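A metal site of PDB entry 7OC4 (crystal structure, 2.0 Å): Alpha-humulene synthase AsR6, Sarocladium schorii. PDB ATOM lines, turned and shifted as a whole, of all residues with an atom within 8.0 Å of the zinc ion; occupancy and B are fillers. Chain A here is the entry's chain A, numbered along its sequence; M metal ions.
The side-chain sulfur (SG) of Cys 89 sits close to the side-chain hydroxyl (OG) of Ser 236 (3.8 Å). ND1 of His 43 sits at hydrogen-bond distance from OD2 of Asp 46.
Four residues have an atom within 4 Å of the zinc ion: His 43, Cys 45, Cys 87 and Cys 89. The nearest printed residue that does not touch the zinc ion is Ser 236 (4.4 Å).
The zinc ion is bound by SG of Cys 89, 2.2 Å away. NE2 of His 43 binds the zinc ion (2.3 Å). SG of Cys 87 is bound to the zinc ion. The side-chain sulfur (SG) of Cys 45 binds the zinc ion (2.5 Å).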
ATOM      1  N   PHE A  31      15.083 -25.031  26.674  1.00  0.00           N
ATOM      2  CA  PHE A  31      15.145 -24.915  28.126  1.00  0.00           C
ATOM      3  C   PHE A  31      13.823 -24.477  28.744  1.00  0.00           C
ATOM      4  O   PHE A  31      13.651 -24.610  29.956  1.00  0.00           O
ATOM      5  CB  PHE A  31      16.271 -23.961  28.554  1.00  0.00           C
ATOM      6  CG  PHE A  31      16.048 -22.521  28.182  1.00  0.00           C
ATOM      7  CD1 PHE A  31      16.479 -22.031  26.970  1.00  0.00           C
ATOM      8  CD2 PHE A  31      15.435 -21.655  29.083  1.00  0.00           C
ATOM      9  CE1 PHE A  31      16.286 -20.705  26.628  1.00  0.00           C
ATOM     10  CE2 PHE A  31      15.240 -20.335  28.753  1.00  0.00           C
ATOM     11  CZ  PHE A  31      15.667 -19.845  27.525  1.00  0.00           C
ATOM     12  N   VAL A  32      12.885 -23.973  27.942  1.00  0.00           N
ATOM     13  CA  VAL A  32      11.537 -23.666  28.407  1.00  0.00           C
ATOM     14  C   VAL A  32      10.620 -24.818  28.020  1.00  0.00           C
ATOM     15  O   VAL A  32      10.522 -25.165  26.840  1.00  0.00           O
ATOM     16  CB  VAL A  32      11.025 -22.334  27.808  1.00  0.00           C
ATOM     17  CG1 VAL A  32       9.563 -22.124  28.186  1.00  0.00           C
ATOM     18  CG2 VAL A  32      11.873 -21.177  28.282  1.00  0.00           C
ATOM     19  N   VAL A  42      20.610 -22.489  25.325  1.00  0.00           N
ATOM     20  CA  VAL A  42      21.291 -21.517  26.177  1.00  0.00           C
ATOM     21  C   VAL A  42      20.314 -20.433  26.574  1.00  0.00           C
ATOM     22  O   VAL A  42      19.594 -19.886  25.731  1.00  0.00           O
ATOM     23  CB  VAL A  42      22.517 -20.924  25.456  1.00  0.00           C
ATOM     24  CG1 VAL A  42      23.251 -19.944  26.366  1.00  0.00           C
ATOM     25  CG2 VAL A  42      23.446 -22.036  25.006  1.00  0.00           C
ATOM     26  N   HIS A  43      20.281 -20.116  27.870  1.00  0.00           N
ATOM     27  CA  HIS A  43      19.456 -19.033  28.416  1.00  0.00           C
ATOM     28  C   HIS A  43      20.284 -17.757  28.383  1.00  0.00           C
ATOM     29  O   HIS A  43      21.168 -17.563  29.221  1.00  0.00           O
ATOM     30  CB  HIS A  43      19.001 -19.377  29.827  1.00  0.00           C
ATOM     31  CG  HIS A  43      17.971 -18.447  30.388  1.00  0.00           C
ATOM     32  ND1 HIS A  43      17.506 -18.544  31.685  1.00  0.00           N
ATOM     33  CD2 HIS A  43      17.323 -17.400  29.831  1.00  0.00           C
ATOM     34  CE1 HIS A  43      16.616 -17.595  31.898  1.00  0.00           C
ATOM     35  NE2 HIS A  43      16.480 -16.889  30.783  1.00  0.00           N
ATOM     36  N   THR A  44      20.009 -16.900  27.405  1.00  0.00           N
ATOM     37  CA  THR A  44      20.844 -15.716  27.204  1.00  0.00           C
ATOM     38  C   THR A  44      20.872 -14.819  28.428  1.00  0.00           C
ATOM     39  O   THR A  44      21.903 -14.189  28.712  1.00  0.00           O
ATOM     40  CB  THR A  44      20.346 -14.924  25.997  1.00  0.00           C
ATOM     41  OG1 THR A  44      18.945 -14.629  26.149  1.00  0.00           O
ATOM     42  CG2 THR A  44      20.555 -15.710  24.711  1.00  0.00           C
ATOM     43  N   CYS A  45      19.766 -14.751  29.171  1.00  0.00           N
ATOM     44  CA  CYS A  45      19.691 -13.852  30.317  1.00  0.00           C
ATOM     45  C   CYS A  45      20.634 -14.252  31.444  1.00  0.00           C
ATOM     46  O   CYS A  45      20.971 -13.410  32.278  1.00  0.00           O
ATOM     47  CB  CYS A  45      18.255 -13.789  30.836  1.00  0.00           C
ATOM     48  SG  CYS A  45      17.053 -13.322  29.576  1.00  0.00           S
ATOM     49  N   ASP A  46      21.052 -15.519  31.492  1.00  0.00           N
ATOM     50  CA  ASP A  46      21.974 -15.991  32.504  1.00  0.00           C
ATOM     51  C   ASP A  46      23.434 -15.907  32.066  1.00  0.00           C
ATOM     52  O   ASP A  46      24.320 -16.377  32.789  1.00  0.00           O
ATOM     53  CB  ASP A  46      21.633 -17.434  32.901  1.00  0.00           C
ATOM     54  CG  ASP A  46      20.473 -17.515  33.873  1.00  0.00           C
ATOM     55  OD1 ASP A  46      20.039 -16.457  34.394  1.00  0.00           O
ATOM     56  OD2 ASP A  46      19.975 -18.644  34.111  1.00  0.00           O
ATOM     57  N   PRO A  85      18.414  -7.395  29.149  1.00  0.00           N
ATOM     58  CA  PRO A  85      16.993  -7.372  28.798  1.00  0.00           C
ATOM     59  C   PRO A  85      16.142  -7.943  29.917  1.00  0.00           C
ATOM     60  O   PRO A  85      16.638  -8.714  30.755  1.00  0.00           O
ATOM     61  CB  PRO A  85      16.923  -8.261  27.548  1.00  0.00           C
ATOM     62  CG  PRO A  85      18.033  -9.232  27.737  1.00  0.00           C
ATOM     63  CD  PRO A  85      19.136  -8.468  28.442  1.00  0.00           C
ATOM     64  N   PRO A  86      14.868  -7.573  29.981  1.00  0.00           N
ATOM     65  CA  PRO A  86      13.936  -8.329  30.827  1.00  0.00           C
ATOM     66  C   PRO A  86      13.715  -9.710  30.230  1.00  0.00           C
ATOM     67  O   PRO A  86      13.641  -9.864  29.003  1.00  0.00           O
ATOM     68  CB  PRO A  86      12.658  -7.489  30.804  1.00  0.00           C
ATOM     69  CG  PRO A  86      12.726  -6.756  29.503  1.00  0.00           C
ATOM     70  CD  PRO A  86      14.190  -6.495  29.245  1.00  0.00           C
ATOM     71  N   CYS A  87      13.643 -10.711  31.096  1.00  0.00           N
ATOM     72  CA  CYS A  87      13.522 -12.088  30.642  1.00  0.00           C
ATOM     73  C   CYS A  87      12.087 -12.343  30.198  1.00  0.00           C
ATOM     74  O   CYS A  87      11.165 -12.355  31.010  1.00  0.00           O
ATOM     75  CB  CYS A  87      13.933 -13.068  31.732  1.00  0.00           C
ATOM     76  SG  CYS A  87      13.718 -14.802  31.261  1.00  0.00           S
ATOM     77  N   THR A  88      11.886 -12.528  28.890  1.00  0.00           N
ATOM     78  CA  THR A  88      10.604 -12.946  28.337  1.00  0.00           C
ATOM     79  C   THR A  88      10.651 -14.353  27.768  1.00  0.00           C
ATOM     80  O   THR A  88       9.717 -14.766  27.079  1.00  0.00           O
ATOM     81  CB  THR A  88      10.151 -11.955  27.262  1.00  0.00           C
ATOM     82  OG1 THR A  88      11.156 -11.836  26.252  1.00  0.00           O
ATOM     83  CG2 THR A  88       9.905 -10.578  27.874  1.00  0.00           C
ATOM     84  N   CYS A  89      11.725 -15.092  28.052  1.00  0.00           N
ATOM     85  CA  CYS A  89      11.920 -16.402  27.424  1.00  0.00           C
ATOM     86  C   CYS A  89      10.817 -17.372  27.812  1.00  0.00           C
ATOM     87  O   CYS A  89      10.364 -18.183  26.992  1.00  0.00           O
ATOM     88  CB  CYS A  89      13.287 -16.972  27.808  1.00  0.00           C
ATOM     89  SG  CYS A  89      14.654 -15.796  27.690  1.00  0.00           S
ATOM     90  N   HIS A  90      10.365 -17.330  29.074  1.00  0.00           N
ATOM     91  CA  HIS A  90       9.417 -18.311  29.575  1.00  0.00           C
ATOM     92  C   HIS A  90       8.056 -18.227  28.892  1.00  0.00           C
ATOM     93  O   HIS A  90       7.235 -19.135  29.091  1.00  0.00           O
ATOM     94  CB  HIS A  90       9.236 -18.157  31.088  1.00  0.00           C
ATOM     95  CG  HIS A  90      10.461 -18.493  31.877  1.00  0.00           C
ATOM     96  ND1 HIS A  90      10.826 -19.787  32.165  1.00  0.00           N
ATOM     97  CD2 HIS A  90      11.408 -17.699  32.439  1.00  0.00           C
ATOM     98  CE1 HIS A  90      11.944 -19.785  32.876  1.00  0.00           C
ATOM     99  NE2 HIS A  90      12.322 -18.528  33.052  1.00  0.00           N
ATOM    100  N   SER A 236      13.966 -11.228  23.975  1.00  0.00           N
ATOM    101  CA  SER A 236      14.303 -12.645  24.123  1.00  0.00           C
ATOM    102  C   SER A 236      13.498 -13.488  23.156  1.00  0.00           C
ATOM    103  O   SER A 236      14.053 -14.355  22.459  1.00  0.00           O
ATOM    104  CB  SER A 236      14.059 -13.097  25.561  1.00  0.00           C
ATOM    105  OG  SER A 236      14.638 -12.202  26.495  1.00  0.00           O
ATOM    106  N   LEU A 237      12.194 -13.261  23.093  1.00  0.00           N
ATOM    107  CA  LEU A 237      11.340 -14.031  22.192  1.00  0.00           C
ATOM    108  C   LEU A 237      11.597 -13.667  20.738  1.00  0.00           C
ATOM    109  O   LEU A 237      11.710 -14.540  19.878  1.00  0.00           O
ATOM    110  CB  LEU A 237       9.869 -13.815  22.549  1.00  0.00           C
ATOM    111  CG  LEU A 237       9.401 -14.355  23.897  1.00  0.00           C
ATOM    112  CD1 LEU A 237       7.927 -14.030  24.100  1.00  0.00           C
ATOM    113  CD2 LEU A 237       9.632 -15.860  24.003  1.00  0.00           C
ATOM    114  N   GLN A 240      14.809 -15.192  19.526  1.00  0.00           N
ATOM    115  CA  GLN A 240      14.671 -16.615  19.293  1.00  0.00           C
ATOM    116  C   GLN A 240      13.947 -16.888  17.976  1.00  0.00           C
ATOM    117  O   GLN A 240      14.316 -17.807  17.243  1.00  0.00           O
ATOM    118  CB  GLN A 240      13.931 -17.277  20.456  1.00  0.00           C
ATOM    119  CG  GLN A 240      14.788 -17.461  21.703  1.00  0.00           C
ATOM    120  CD  GLN A 240      14.083 -18.185  22.827  1.00  0.00           C
ATOM    121  OE1 GLN A 240      12.873 -18.436  22.758  1.00  0.00           O
ATOM    122  NE2 GLN A 240      14.812 -18.532  23.876  1.00  0.00           N
HETATM  123 ZN    ZN M   1      15.413 -15.145  29.695  1.00  0.00          ZN
